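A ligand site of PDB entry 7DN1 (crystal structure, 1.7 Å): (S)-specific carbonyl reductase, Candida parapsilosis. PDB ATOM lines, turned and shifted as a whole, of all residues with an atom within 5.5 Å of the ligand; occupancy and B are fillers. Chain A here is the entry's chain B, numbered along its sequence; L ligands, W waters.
The backbone carbonyl oxygen of Gly 218 sits close to an oxygen (O14) of the ligand. Ser 43 touches the ligand. Tyr 66 touches the ligand. Cys 91 touches the ligand (O to C9, 3.2 Å). Ser 94 touches the ligand (OG to N3, 3.97 Å). CA of Ala 120 touches O4 of the ligand, at 3.7 Å. Val 122 touches the ligand. CD2 of Leu 144 touches N2 of the ligand, at 3.3 Å. Thr 171 touches the ligand (CG2 to O11, 3.5 Å). Ser 172 touches the ligand (O to C21, 3.2 Å). OG of Ser 173 touches C20 of the ligand, at 3.4 Å. Pro 217 touches the ligand. C of Tyr 219 touches O14 of the ligand, 3.8 Å away.
Water W3 lies within hydrogen-bond range of N of Gly 42 (2.8 Å) and N5 of the ligand (3.0 Å). Water W1 lies within hydrogen-bond range of OG of Ser 173 (2.7 Å) and OH of Tyr 188 (2.8 Å).
The backbone carbonyl oxygen (O) of Gly 42 is in hydrogen-bond range of the side-chain amide nitrogen (ND2) of Asn 119, 3.4 Å away. OG of Ser 225 lies within hydrogen-bond range of O of Ile 220 (2.9 Å). O of His 69 is in hydrogen-bond range of OG of Ser 44, at 3.1 Å. O of Ser 173 lies within hydrogen-bond range of OG of Ser 216 (3.4 Å). OG of Ser 172 lies within hydrogen-bond range of O of Lys 192 (3.0 Å). OG of Ser 43 is in hydrogen-bond range of N of Trp 65 (3.0 Å). The side-chain amide oxygen of Asn 119 sits at hydrogen-bond distance from the side-chain hydroxyl of Thr 171 (3.0 Å). O of Trp 65 lies within hydrogen-bond range of N of Ser 44.
An oxygen (O15) of the ligand sits at hydrogen-bond distance from the backbone NH (N) of Asn 67, 2.9 Å away. N of Gly 121 sits at hydrogen-bond distance from O4 of the ligand, at 3.5 Å. N of His 69 is in hydrogen-bond range of O15 of the ligand (3.0 Å). O5 of the ligand lies close to N of Ser 44. The backbone NH of Ser 68 is in hydrogen-bond range of an oxygen (O17) of the ligand (2.8 Å). A ring nitrogen (ND1) of His 69 lies within hydrogen-bond range of an oxygen (O16) of the ligand, at 2.9 Å. The side-chain hydroxyl (OH) of Tyr 188 sits at hydrogen-bond distance from an oxygen (O13) of the ligand (2.6 Å). An oxygen (O14) of the ligand lies within hydrogen-bond range of the backbone NH (N) of Ile 220 (2.9 Å). The backbone carbonyl oxygen of Gly 42 lies within hydrogen-bond range of an oxygen (O5) of the ligand (3.1 Å). An oxygen (O5) of the ligand sits at hydrogen-bond distance from the backbone NH (N) of Gly 45 (3.0 Å). N4 of the ligand is in hydrogen-bond range of N of Ile 93 (3.1 Å). The backbone NH of Ile 47 is in hydrogen-bond range of an oxygen (O8) of the ligand (2.9 Å). The backbone NH (N) of Gly 46 lies within hydrogen-bond range of an oxygen (O1) of the ligand, at 3.0 Å. A nitrogen (N3) of the ligand sits at hydrogen-bond distance from the side-chain amide oxygen (OD1) of Asn 92 (2.9 Å). The side-chain amino group (NZ) of Lys 192 is in hydrogen-bond range of an oxygen (O12) of the ligand, 3.1 Å away. The backbone carbonyl oxygen of Asn 119 sits at hydrogen-bond distance from an oxygen (O12) of the ligand (2.8 Å). OG of Ser 44 sits at hydrogen-bond distance from O15 of the ligand. A nitrogen (N7) of the ligand is in hydrogen-bond range of the side-chain hydroxyl (OG1) of Thr 222 (3.2 Å).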
ATOM      1  N   GLY A  42     -29.895 -10.084  -9.255  1.00  0.00           N
ATOM      2  CA  GLY A  42     -29.134  -9.193  -8.391  1.00  0.00           C
ATOM      3  C   GLY A  42     -29.869  -7.933  -8.003  1.00  0.00           C
ATOM      4  O   GLY A  42     -29.255  -6.879  -7.829  1.00  0.00           O
ATOM      5  N   SER A  43     -31.194  -8.009  -7.850  1.00  0.00           N
ATOM      6  CA  SER A  43     -31.979  -6.826  -7.541  1.00  0.00           C
ATOM      7  C   SER A  43     -32.223  -6.662  -6.036  1.00  0.00           C
ATOM      8  O   SER A  43     -33.046  -5.832  -5.642  1.00  0.00           O
ATOM      9  CB  SER A  43     -33.245  -6.824  -8.412  1.00  0.00           C
ATOM     10  OG  SER A  43     -34.126  -7.927  -8.235  1.00  0.00           O
ATOM     11  N   SER A  44     -31.472  -7.393  -5.215  1.00  0.00           N
ATOM     12  CA  SER A  44     -31.148  -6.946  -3.854  1.00  0.00           C
ATOM     13  C   SER A  44     -30.265  -5.716  -3.879  1.00  0.00           C
ATOM     14  O   SER A  44     -30.415  -4.808  -3.058  1.00  0.00           O
ATOM     15  CB  SER A  44     -30.408  -8.025  -3.083  1.00  0.00           C
ATOM     16  OG  SER A  44     -31.161  -9.179  -2.942  1.00  0.00           O
ATOM     17  N   GLY A  45     -29.279  -5.708  -4.780  1.00  0.00           N
ATOM     18  CA  GLY A  45     -28.199  -4.761  -4.723  1.00  0.00           C
ATOM     19  C   GLY A  45     -28.505  -3.474  -5.447  1.00  0.00           C
ATOM     20  O   GLY A  45     -29.604  -3.255  -5.960  1.00  0.00           O
ATOM     21  N   GLY A  46     -27.495  -2.610  -5.494  1.00  0.00           N
ATOM     22  CA  GLY A  46     -27.643  -1.241  -5.937  1.00  0.00           C
ATOM     23  C   GLY A  46     -28.235  -1.093  -7.313  1.00  0.00           C
ATOM     24  O   GLY A  46     -29.329  -0.560  -7.470  1.00  0.00           O
ATOM     25  N   ILE A  47     -27.507  -1.570  -8.329  1.00  0.00           N
ATOM     26  CA  ILE A  47     -27.948  -1.366  -9.693  1.00  0.00           C
ATOM     27  C   ILE A  47     -29.244  -2.133  -9.952  1.00  0.00           C
ATOM     28  O   ILE A  47     -30.183  -1.591 -10.557  1.00  0.00           O
ATOM     29  CB  ILE A  47     -26.833  -1.762 -10.672  1.00  0.00           C
ATOM     30  CG1 ILE A  47     -25.617  -0.829 -10.507  1.00  0.00           C
ATOM     31  CG2 ILE A  47     -27.323  -1.740 -12.126  1.00  0.00           C
ATOM     32  CD1 ILE A  47     -24.457  -1.177 -11.396  1.00  0.00           C
ATOM     33  N   GLY A  48     -29.332  -3.374  -9.467  1.00  0.00           N
ATOM     34  CA  GLY A  48     -30.486  -4.208  -9.771  1.00  0.00           C
ATOM     35  C   GLY A  48     -31.777  -3.636  -9.213  1.00  0.00           C
ATOM     36  O   GLY A  48     -32.813  -3.669  -9.882  1.00  0.00           O
ATOM     37  N   TRP A  65     -34.706 -10.830  -7.608  1.00  0.00           N
ATOM     38  CA  TRP A  65     -33.825 -11.936  -7.267  1.00  0.00           C
ATOM     39  C   TRP A  65     -32.914 -11.528  -6.133  1.00  0.00           C
ATOM     40  O   TRP A  65     -32.398 -10.413  -6.120  1.00  0.00           O
ATOM     41  CB  TRP A  65     -32.913 -12.354  -8.423  1.00  0.00           C
ATOM     42  CG  TRP A  65     -33.537 -12.868  -9.655  1.00  0.00           C
ATOM     43  CD1 TRP A  65     -34.508 -12.272 -10.412  1.00  0.00           C
ATOM     44  CD2 TRP A  65     -33.195 -14.081 -10.336  1.00  0.00           C
ATOM     45  NE1 TRP A  65     -34.788 -13.049 -11.509  1.00  0.00           N
ATOM     46  CE2 TRP A  65     -33.994 -14.163 -11.485  1.00  0.00           C
ATOM     47  CE3 TRP A  65     -32.290 -15.109 -10.074  1.00  0.00           C
ATOM     48  CZ2 TRP A  65     -33.932 -15.235 -12.372  1.00  0.00           C
ATOM     49  CZ3 TRP A  65     -32.215 -16.178 -10.957  1.00  0.00           C
ATOM     50  CH2 TRP A  65     -33.033 -16.226 -12.092  1.00  0.00           C
ATOM     51  N   TYR A  66     -32.656 -12.469  -5.219  1.00  0.00           N
ATOM     52  CA  TYR A  66     -31.699 -12.253  -4.154  1.00  0.00           C
ATOM     53  C   TYR A  66     -30.976 -13.545  -3.840  1.00  0.00           C
ATOM     54  O   TYR A  66     -31.379 -14.638  -4.247  1.00  0.00           O
ATOM     55  CB  TYR A  66     -32.371 -11.702  -2.887  1.00  0.00           C
ATOM     56  CG  TYR A  66     -33.328 -12.615  -2.162  1.00  0.00           C
ATOM     57  CD1 TYR A  66     -32.892 -13.427  -1.126  1.00  0.00           C
ATOM     58  CD2 TYR A  66     -34.671 -12.642  -2.507  1.00  0.00           C
ATOM     59  CE1 TYR A  66     -33.773 -14.237  -0.445  1.00  0.00           C
ATOM     60  CE2 TYR A  66     -35.556 -13.458  -1.834  1.00  0.00           C
ATOM     61  CZ  TYR A  66     -35.098 -14.253  -0.808  1.00  0.00           C
ATOM     62  OH  TYR A  66     -35.983 -15.069  -0.134  1.00  0.00           O
ATOM     63  N   ASN A  67     -29.853 -13.395  -3.138  1.00  0.00           N
ATOM     64  CA  ASN A  67     -29.116 -14.540  -2.626  1.00  0.00           C
ATOM     65  C   ASN A  67     -29.015 -14.448  -1.115  1.00  0.00           C
ATOM     66  O   ASN A  67     -29.811 -15.066  -0.398  1.00  0.00           O
ATOM     67  CB  ASN A  67     -27.727 -14.623  -3.263  1.00  0.00           C
ATOM     68  CG  ASN A  67     -27.046 -15.949  -2.981  1.00  0.00           C
ATOM     69  OD1 ASN A  67     -27.705 -16.988  -2.902  1.00  0.00           O
ATOM     70  ND2 ASN A  67     -25.727 -15.928  -2.843  1.00  0.00           N
ATOM     71  N   SER A  68     -28.079 -13.643  -0.607  1.00  0.00           N
ATOM     72  CA  SER A  68     -27.836 -13.586   0.836  1.00  0.00           C
ATOM     73  C   SER A  68     -28.612 -12.480   1.548  1.00  0.00           C
ATOM     74  O   SER A  68     -28.541 -12.406   2.782  1.00  0.00           O
ATOM     75  CB  SER A  68     -26.340 -13.424   1.114  1.00  0.00           C
ATOM     76  OG  SER A  68     -25.635 -14.598   0.763  1.00  0.00           O
ATOM     77  N   HIS A  69     -29.360 -11.639   0.835  1.00  0.00           N
ATOM     78  CA  HIS A  69     -30.079 -10.530   1.462  1.00  0.00           C
ATOM     79  C   HIS A  69     -31.535 -10.532   1.029  1.00  0.00           C
ATOM     80  O   HIS A  69     -31.872  -9.971  -0.037  1.00  0.00           O
ATOM     81  CB  HIS A  69     -29.411  -9.197   1.141  1.00  0.00           C
ATOM     82  CG  HIS A  69     -28.023  -9.079   1.692  1.00  0.00           C
ATOM     83  ND1 HIS A  69     -26.892  -9.140   0.905  1.00  0.00           N
ATOM     84  CD2 HIS A  69     -27.588  -8.877   2.960  1.00  0.00           C
ATOM     85  CE1 HIS A  69     -25.825  -8.988   1.662  1.00  0.00           C
ATOM     86  NE2 HIS A  69     -26.213  -8.839   2.911  1.00  0.00           N
ATOM     87  N   PRO A  70     -32.441 -11.125   1.816  1.00  0.00           N
ATOM     88  CA  PRO A  70     -33.824 -11.291   1.373  1.00  0.00           C
ATOM     89  C   PRO A  70     -34.472  -9.977   0.950  1.00  0.00           C
ATOM     90  O   PRO A  70     -34.378  -8.963   1.646  1.00  0.00           O
ATOM     91  CB  PRO A  70     -34.531 -11.877   2.602  1.00  0.00           C
ATOM     92  CG  PRO A  70     -33.453 -12.425   3.467  1.00  0.00           C
ATOM     93  CD  PRO A  70     -32.113 -11.954   2.987  1.00  0.00           C
ATOM     94  N   CYS A  91     -31.961 -17.342  -5.128  1.00  0.00           N
ATOM     95  CA  CYS A  91     -31.261 -18.187  -6.081  1.00  0.00           C
ATOM     96  C   CYS A  91     -29.767 -17.900  -6.045  1.00  0.00           C
ATOM     97  O   CYS A  91     -29.347 -16.742  -6.112  1.00  0.00           O
ATOM     98  CB  CYS A  91     -31.785 -17.984  -7.518  1.00  0.00           C
ATOM     99  SG  CYS A  91     -31.043 -19.074  -8.778  1.00  0.00           S
ATOM    100  N   ASN A  92     -28.970 -18.968  -5.987  1.00  0.00           N
ATOM    101  CA  ASN A  92     -27.536 -18.903  -6.192  1.00  0.00           C
ATOM    102  C   ASN A  92     -27.269 -19.129  -7.681  1.00  0.00           C
ATOM    103  O   ASN A  92     -27.418 -20.243  -8.187  1.00  0.00           O
ATOM    104  CB  ASN A  92     -26.827 -19.942  -5.326  1.00  0.00           C
ATOM    105  CG  ASN A  92     -25.329 -19.973  -5.528  1.00  0.00           C
ATOM    106  OD1 ASN A  92     -24.757 -19.125  -6.211  1.00  0.00           O
ATOM    107  ND2 ASN A  92     -24.678 -20.968  -4.937  1.00  0.00           N
ATOM    108  N   ILE A  93     -26.883 -18.069  -8.392  1.00  0.00           N
ATOM    109  CA  ILE A  93     -26.740 -18.165  -9.834  1.00  0.00           C
ATOM    110  C   ILE A  93     -25.522 -18.979 -10.270  1.00  0.00           C
ATOM    111  O   ILE A  93     -25.456 -19.400 -11.425  1.00  0.00           O
ATOM    112  CB  ILE A  93     -26.802 -16.727 -10.422  1.00  0.00           C
ATOM    113  CG1 ILE A  93     -28.240 -16.211 -10.341  1.00  0.00           C
ATOM    114  CG2 ILE A  93     -26.367 -16.656 -11.845  1.00  0.00           C
ATOM    115  CD1 ILE A  93     -28.369 -14.732 -10.603  1.00  0.00           C
ATOM    116  N   SER A  94     -24.592 -19.278  -9.360  1.00  0.00           N
ATOM    117  CA  SER A  94     -23.549 -20.235  -9.723  1.00  0.00           C
ATOM    118  C   SER A  94     -24.054 -21.673  -9.804  1.00  0.00           C
ATOM    119  O   SER A  94     -23.312 -22.542 -10.273  1.00  0.00           O
ATOM    120  CB  SER A  94     -22.372 -20.187  -8.744  1.00  0.00           C
ATOM    121  OG  SER A  94     -21.938 -18.865  -8.534  1.00  0.00           O
ATOM    122  N   ASN A 119     -27.817  -9.407 -14.164  1.00  0.00           N
ATOM    123  CA  ASN A 119     -27.114  -8.326 -13.502  1.00  0.00           C
ATOM    124  C   ASN A 119     -26.315  -8.743 -12.269  1.00  0.00           C
ATOM    125  O   ASN A 119     -25.349  -8.058 -11.921  1.00  0.00           O
ATOM    126  CB  ASN A 119     -28.119  -7.224 -13.138  1.00  0.00           C
ATOM    127  CG  ASN A 119     -27.551  -6.221 -12.165  1.00  0.00           C
ATOM    128  OD1 ASN A 119     -26.758  -5.345 -12.538  1.00  0.00           O
ATOM    129  ND2 ASN A 119     -27.925  -6.352 -10.920  1.00  0.00           N
ATOM    130  N   ALA A 120     -26.677  -9.849 -11.607  1.00  0.00           N
ATOM    131  CA  ALA A 120     -25.966 -10.292 -10.414  1.00  0.00           C
ATOM    132  C   ALA A 120     -24.484 -10.531 -10.692  1.00  0.00           C
ATOM    133  O   ALA A 120     -24.111 -11.023 -11.769  1.00  0.00           O
ATOM    134  CB  ALA A 120     -26.610 -11.573  -9.889  1.00  0.00           C
ATOM    135  N   GLY A 121     -23.634 -10.187  -9.708  1.00  0.00           N
ATOM    136  CA  GLY A 121     -22.195 -10.391  -9.828  1.00  0.00           C
ATOM    137  C   GLY A 121     -21.468 -10.022  -8.541  1.00  0.00           C
ATOM    138  O   GLY A 121     -22.051  -9.483  -7.593  1.00  0.00           O
ATOM    139  N   VAL A 122     -20.175 -10.350  -8.525  1.00  0.00           N
ATOM    140  CA  VAL A 122     -19.275 -10.048  -7.407  1.00  0.00           C
ATOM    141  C   VAL A 122     -17.989  -9.447  -7.944  1.00  0.00           C
ATOM    142  O   VAL A 122     -17.622  -9.678  -9.101  1.00  0.00           O
ATOM    143  CB  VAL A 122     -18.979 -11.307  -6.551  1.00  0.00           C
ATOM    144  CG1 VAL A 122     -20.247 -11.854  -5.914  1.00  0.00           C
ATOM    145  CG2 VAL A 122     -18.284 -12.368  -7.394  1.00  0.00           C
ATOM    146  N   LEU A 144     -19.607 -17.115 -11.088  1.00  0.00           N
ATOM    147  CA  LEU A 144     -20.754 -16.240 -10.918  1.00  0.00           C
ATOM    148  C   LEU A 144     -20.881 -15.212 -12.041  1.00  0.00           C
ATOM    149  O   LEU A 144     -21.975 -15.000 -12.565  1.00  0.00           O
ATOM    150  CB  LEU A 144     -20.702 -15.527  -9.560  1.00  0.00           C
ATOM    151  CG  LEU A 144     -21.918 -14.620  -9.452  1.00  0.00           C
ATOM    152  CD1 LEU A 144     -23.199 -15.453  -9.595  1.00  0.00           C
ATOM    153  CD2 LEU A 144     -21.918 -13.914  -8.141  1.00  0.00           C
ATOM    154  N   THR A 171     -25.686  -6.938 -17.675  1.00  0.00           N
ATOM    155  CA  THR A 171     -24.832  -5.911 -17.072  1.00  0.00           C
ATOM    156  C   THR A 171     -23.397  -6.374 -17.200  1.00  0.00           C
ATOM    157  O   THR A 171     -22.969  -7.317 -16.536  1.00  0.00           O
ATOM    158  CB  THR A 171     -25.170  -5.658 -15.616  1.00  0.00           C
ATOM    159  OG1 THR A 171     -26.545  -5.258 -15.490  1.00  0.00           O
ATOM    160  CG2 THR A 171     -24.267  -4.542 -15.060  1.00  0.00           C
ATOM    161  N   SER A 172     -22.625  -5.687 -18.030  1.00  0.00           N
ATOM    162  CA  SER A 172     -21.195  -5.922 -18.124  1.00  0.00           C
ATOM    163  C   SER A 172     -20.490  -4.863 -17.263  1.00  0.00           C
ATOM    164  O   SER A 172     -20.928  -4.634 -16.147  1.00  0.00           O
ATOM    165  CB  SER A 172     -20.771  -5.954 -19.592  1.00  0.00           C
ATOM    166  OG  SER A 172     -19.395  -6.261 -19.633  1.00  0.00           O
ATOM    167  N   SER A 173     -19.448  -4.214 -17.753  1.00  0.00           N
ATOM    168  CA  SER A 173     -18.729  -3.220 -16.988  1.00  0.00           C
ATOM    169  C   SER A 173     -17.760  -2.570 -17.940  1.00  0.00           C
ATOM    170  O   SER A 173     -17.392  -3.150 -18.969  1.00  0.00           O
ATOM    171  CB  SER A 173     -17.944  -3.828 -15.804  1.00  0.00           C
ATOM    172  OG  SER A 173     -17.050  -2.851 -15.295  1.00  0.00           O
ATOM    173  N   MET A 174     -17.316  -1.378 -17.582  1.00  0.00           N
ATOM    174  CA  MET A 174     -16.268  -0.756 -18.360  1.00  0.00           C
ATOM    175  C   MET A 174     -15.039  -1.650 -18.325  1.00  0.00           C
ATOM    176  O   MET A 174     -14.200  -1.646 -19.235  1.00  0.00           O
ATOM    177  CB  MET A 174     -15.991   0.614 -17.778  1.00  0.00           C
ATOM    178  CG  MET A 174     -15.378   0.628 -16.429  1.00  0.00           C
ATOM    179  SD  MET A 174     -15.309   2.416 -16.319  1.00  0.00           S
ATOM    180  CE  MET A 174     -14.193   2.667 -17.573  1.00  0.00           C
ATOM    181  N   TYR A 188     -11.799 -10.373 -12.897  1.00  0.00           N
ATOM    182  CA  TYR A 188     -13.059  -9.675 -13.115  1.00  0.00           C
ATOM    183  C   TYR A 188     -13.121  -9.070 -14.506  1.00  0.00           C
ATOM    184  O   TYR A 188     -14.156  -9.161 -15.189  1.00  0.00           O
ATOM    185  CB  TYR A 188     -13.230  -8.594 -12.055  1.00  0.00           C
ATOM    186  CG  TYR A 188     -14.487  -7.748 -12.162  1.00  0.00           C
ATOM    187  CD1 TYR A 188     -14.477  -6.525 -12.817  1.00  0.00           C
ATOM    188  CD2 TYR A 188     -15.671  -8.153 -11.547  1.00  0.00           C
ATOM    189  CE1 TYR A 188     -15.623  -5.727 -12.886  1.00  0.00           C
ATOM    190  CE2 TYR A 188     -16.808  -7.374 -11.608  1.00  0.00           C
ATOM    191  CZ  TYR A 188     -16.788  -6.166 -12.285  1.00  0.00           C
ATOM    192  OH  TYR A 188     -17.930  -5.417 -12.337  1.00  0.00           O
ATOM    193  N   LYS A 192     -15.876  -9.936 -17.447  1.00  0.00           N
ATOM    194  CA  LYS A 192     -16.787  -8.951 -18.021  1.00  0.00           C
ATOM    195  C   LYS A 192     -16.596  -8.813 -19.527  1.00  0.00           C
ATOM    196  O   LYS A 192     -17.562  -8.583 -20.252  1.00  0.00           O
ATOM    197  CB  LYS A 192     -16.617  -7.593 -17.333  1.00  0.00           C
ATOM    198  CG  LYS A 192     -17.125  -7.608 -15.881  1.00  0.00           C
ATOM    199  CD  LYS A 192     -18.630  -7.884 -15.866  1.00  0.00           C
ATOM    200  CE  LYS A 192     -19.238  -7.632 -14.486  1.00  0.00           C
ATOM    201  NZ  LYS A 192     -20.738  -7.867 -14.515  1.00  0.00           N
ATOM    202  N   SER A 216     -22.678  -1.252 -19.989  1.00  0.00           N
ATOM    203  CA  SER A 216     -21.348  -1.283 -19.372  1.00  0.00           C
ATOM    204  C   SER A 216     -21.201  -0.044 -18.486  1.00  0.00           C
ATOM    205  O   SER A 216     -20.716   0.993 -18.945  1.00  0.00           O
ATOM    206  CB  SER A 216     -20.257  -1.314 -20.436  1.00  0.00           C
ATOM    207  OG  SER A 216     -20.129  -2.622 -20.976  1.00  0.00           O
ATOM    208  N   PRO A 217     -21.591  -0.115 -17.206  1.00  0.00           N
ATOM    209  CA  PRO A 217     -21.411   1.047 -16.326  1.00  0.00           C
ATOM    210  C   PRO A 217     -19.954   1.297 -16.007  1.00  0.00           C
ATOM    211  O   PRO A 217     -19.121   0.385 -16.021  1.00  0.00           O
ATOM    212  CB  PRO A 217     -22.190   0.664 -15.048  1.00  0.00           C
ATOM    213  CG  PRO A 217     -22.987  -0.604 -15.415  1.00  0.00           C
ATOM    214  CD  PRO A 217     -22.221  -1.258 -16.531  1.00  0.00           C
ATOM    215  N   GLY A 218     -19.669   2.577 -15.753  1.00  0.00           N
ATOM    216  CA  GLY A 218     -18.432   2.991 -15.106  1.00  0.00           C
ATOM    217  C   GLY A 218     -18.502   2.853 -13.599  1.00  0.00           C
ATOM    218  O   GLY A 218     -19.152   1.954 -13.063  1.00  0.00           O
ATOM    219  N   TYR A 219     -17.793   3.740 -12.903  1.00  0.00           N
ATOM    220  CA  TYR A 219     -17.827   3.725 -11.445  1.00  0.00           C
ATOM    221  C   TYR A 219     -19.159   4.292 -10.966  1.00  0.00           C
ATOM    222  O   TYR A 219     -19.425   5.481 -11.158  1.00  0.00           O
ATOM    223  CB  TYR A 219     -16.660   4.540 -10.884  1.00  0.00           C
ATOM    224  CG  TYR A 219     -15.344   3.835 -11.103  1.00  0.00           C
ATOM    225  CD1 TYR A 219     -15.042   2.667 -10.417  1.00  0.00           C
ATOM    226  CD2 TYR A 219     -14.422   4.309 -12.031  1.00  0.00           C
ATOM    227  CE1 TYR A 219     -13.838   1.977 -10.651  1.00  0.00           C
ATOM    228  CE2 TYR A 219     -13.231   3.646 -12.262  1.00  0.00           C
ATOM    229  CZ  TYR A 219     -12.953   2.477 -11.576  1.00  0.00           C
ATOM    230  OH  TYR A 219     -11.745   1.822 -11.795  1.00  0.00           O
ATOM    231  N   ILE A 220     -19.976   3.452 -10.327  1.00  0.00           N
ATOM    232  CA  ILE A 220     -21.285   3.858  -9.819  1.00  0.00           C
ATOM    233  C   ILE A 220     -21.250   3.849  -8.297  1.00  0.00           C
ATOM    234  O   ILE A 220     -20.806   2.871  -7.684  1.00  0.00           O
ATOM    235  CB  ILE A 220     -22.389   2.918 -10.330  1.00  0.00           C
ATOM    236  CG1 ILE A 220     -22.301   2.760 -11.846  1.00  0.00           C
ATOM    237  CG2 ILE A 220     -23.773   3.425  -9.888  1.00  0.00           C
ATOM    238  CD1 ILE A 220     -22.520   4.057 -12.611  1.00  0.00           C
ATOM    239  N   ALA A 221     -21.780   4.916  -7.693  1.00  0.00           N
ATOM    240  CA  ALA A 221     -21.811   5.043  -6.240  1.00  0.00           C
ATOM    241  C   ALA A 221     -22.850   4.117  -5.606  1.00  0.00           C
ATOM    242  O   ALA A 221     -23.831   4.597  -5.036  1.00  0.00           O
ATOM    243  CB  ALA A 221     -22.111   6.486  -5.842  1.00  0.00           C
ATOM    244  N   THR A 222     -22.652   2.806  -5.720  1.00  0.00           N
ATOM    245  CA  THR A 222     -23.349   1.848  -4.881  1.00  0.00           C
ATOM    246  C   THR A 222     -22.578   1.647  -3.579  1.00  0.00           C
ATOM    247  O   THR A 222     -21.440   2.097  -3.432  1.00  0.00           O
ATOM    248  CB  THR A 222     -23.518   0.502  -5.604  1.00  0.00           C
ATOM    249  OG1 THR A 222     -22.231  -0.100  -5.796  1.00  0.00           O
ATOM    250  CG2 THR A 222     -24.265   0.662  -6.930  1.00  0.00           C
ATOM    251  N   ILE A 224     -21.266  -1.029  -2.392  1.00  0.00           N
ATOM    252  CA  ILE A 224     -20.098  -1.900  -2.538  1.00  0.00           C
ATOM    253  C   ILE A 224     -18.825  -1.089  -2.785  1.00  0.00           C
ATOM    254  O   ILE A 224     -17.833  -1.244  -2.072  1.00  0.00           O
ATOM    255  CB  ILE A 224     -20.333  -2.885  -3.692  1.00  0.00           C
ATOM    256  N   SER A 225     -18.856  -0.208  -3.784  1.00  0.00           N
ATOM    257  CA  SER A 225     -17.678   0.519  -4.228  1.00  0.00           C
ATOM    258  C   SER A 225     -17.517   1.871  -3.531  1.00  0.00           C
ATOM    259  O   SER A 225     -16.755   2.714  -4.023  1.00  0.00           O
ATOM    260  CB  SER A 225     -17.734   0.720  -5.734  1.00  0.00           C
ATOM    261  OG  SER A 225     -18.601   1.791  -6.073  1.00  0.00           O
HETATM  262  P1  LIG L   1     -24.074  -5.073  -5.284  1.00  0.00           P
HETATM  263  O1  LIG L   1     -24.884  -3.929  -4.659  1.00  0.00           O
HETATM  264  O2  LIG L   1     -23.137  -5.841  -4.407  1.00  0.00           O
HETATM  265  O3  LIG L   1     -25.154  -6.159  -5.922  1.00  0.00           O
HETATM  266  C1  LIG L   1     -24.743  -7.509  -5.876  1.00  0.00           C
HETATM  267  C2  LIG L   1     -25.998  -8.302  -6.245  1.00  0.00           C
HETATM  268  O4  LIG L   1     -25.460  -9.691  -6.808  1.00  0.00           O
HETATM  269  C3  LIG L   1     -26.687  -8.536  -5.156  1.00  0.00           C
HETATM  270  O5  LIG L   1     -28.147  -8.448  -5.422  1.00  0.00           O
HETATM  271  C4  LIG L   1     -26.335 -10.005  -4.771  1.00  0.00           C
HETATM  272  O6  LIG L   1     -27.370 -10.597  -4.125  1.00  0.00           O
HETATM  273  C5  LIG L   1     -26.204 -10.591  -6.168  1.00  0.00           C
HETATM  274  N1  LIG L   1     -25.477 -11.835  -6.086  1.00  0.00           N
HETATM  275  C6  LIG L   1     -24.243 -11.703  -5.606  1.00  0.00           C
HETATM  276  N2  LIG L   1     -23.738 -12.942  -5.591  1.00  0.00           N
HETATM  277  C7  LIG L   1     -24.667 -13.796  -6.045  1.00  0.00           C
HETATM  278  C8  LIG L   1     -24.672 -15.144  -6.234  1.00  0.00           C
HETATM  279  N3  LIG L   1     -23.857 -16.386  -6.096  1.00  0.00           N
HETATM  280  N4  LIG L   1     -25.751 -15.745  -6.709  1.00  0.00           N
HETATM  281  C9  LIG L   1     -26.847 -15.031  -7.027  1.00  0.00           C
HETATM  282  N5  LIG L   1     -26.859 -13.699  -6.844  1.00  0.00           N
HETATM  283  C10 LIG L   1     -25.753 -13.101  -6.355  1.00  0.00           C
HETATM  284  O7  LIG L   1     -23.204  -4.501  -6.567  1.00  0.00           O
HETATM  285  P2  LIG L   1     -23.799  -3.615  -7.817  1.00  0.00           P
HETATM  286  O8  LIG L   1     -25.279  -3.341  -7.827  1.00  0.00           O
HETATM  287  O9  LIG L   1     -22.976  -2.331  -7.925  1.00  0.00           O
HETATM  288  O10 LIG L   1     -23.428  -4.555  -9.147  1.00  0.00           O
HETATM  289  C11 LIG L   1     -24.388  -5.363  -9.746  1.00  0.00           C
HETATM  290  C12 LIG L   1     -23.732  -5.681 -11.187  1.00  0.00           C
HETATM  291  O11 LIG L   1     -23.225  -4.349 -11.764  1.00  0.00           O
HETATM  292  C13 LIG L   1     -22.717  -6.442 -11.084  1.00  0.00           C
HETATM  293  O12 LIG L   1     -22.694  -7.400 -12.213  1.00  0.00           O
HETATM  294  C14 LIG L   1     -21.391  -5.479 -11.265  1.00  0.00           C
HETATM  295  O13 LIG L   1     -20.267  -6.316 -11.701  1.00  0.00           O
HETATM  296  C15 LIG L   1     -21.773  -4.679 -12.176  1.00  0.00           C
HETATM  297  N6  LIG L   1     -21.044  -3.387 -12.185  1.00  0.00           N
HETATM  298  C16 LIG L   1     -21.021  -2.574 -11.038  1.00  0.00           C
HETATM  299  C17 LIG L   1     -20.360  -1.214 -11.070  1.00  0.00           C
HETATM  300  C18 LIG L   1     -20.349  -0.315  -9.867  1.00  0.00           C
HETATM  301  O14 LIG L   1     -19.654   0.640  -9.909  1.00  0.00           O
HETATM  302  N7  LIG L   1     -21.178  -0.618  -8.722  1.00  0.00           N
HETATM  303  C19 LIG L   1     -19.486  -0.761 -12.261  1.00  0.00           C
HETATM  304  C20 LIG L   1     -19.678  -1.630 -13.530  1.00  0.00           C
HETATM  305  C21 LIG L   1     -20.415  -2.988 -13.406  1.00  0.00           C
HETATM  306  P3  LIG L   1     -27.407 -10.643  -2.447  1.00  0.00           P
HETATM  307  O15 LIG L   1     -28.842 -10.872  -2.039  1.00  0.00           O
HETATM  308  O16 LIG L   1     -26.916  -9.328  -1.959  1.00  0.00           O
HETATM  309  O17 LIG L   1     -26.518 -11.767  -1.953  1.00  0.00           O
HETATM  310  O   HOH W   1     -17.061  -2.801 -12.546  1.00  0.00           O
HETATM  311  O   HOH W   2     -21.587 -15.173  -4.646  1.00  0.00           O
HETATM  312  O   HOH W   3     -29.317 -12.320  -7.751  1.00  0.00           O
HETATM  313  O   HOH W   4     -27.352  -4.797  -8.455  1.00  0.00           O
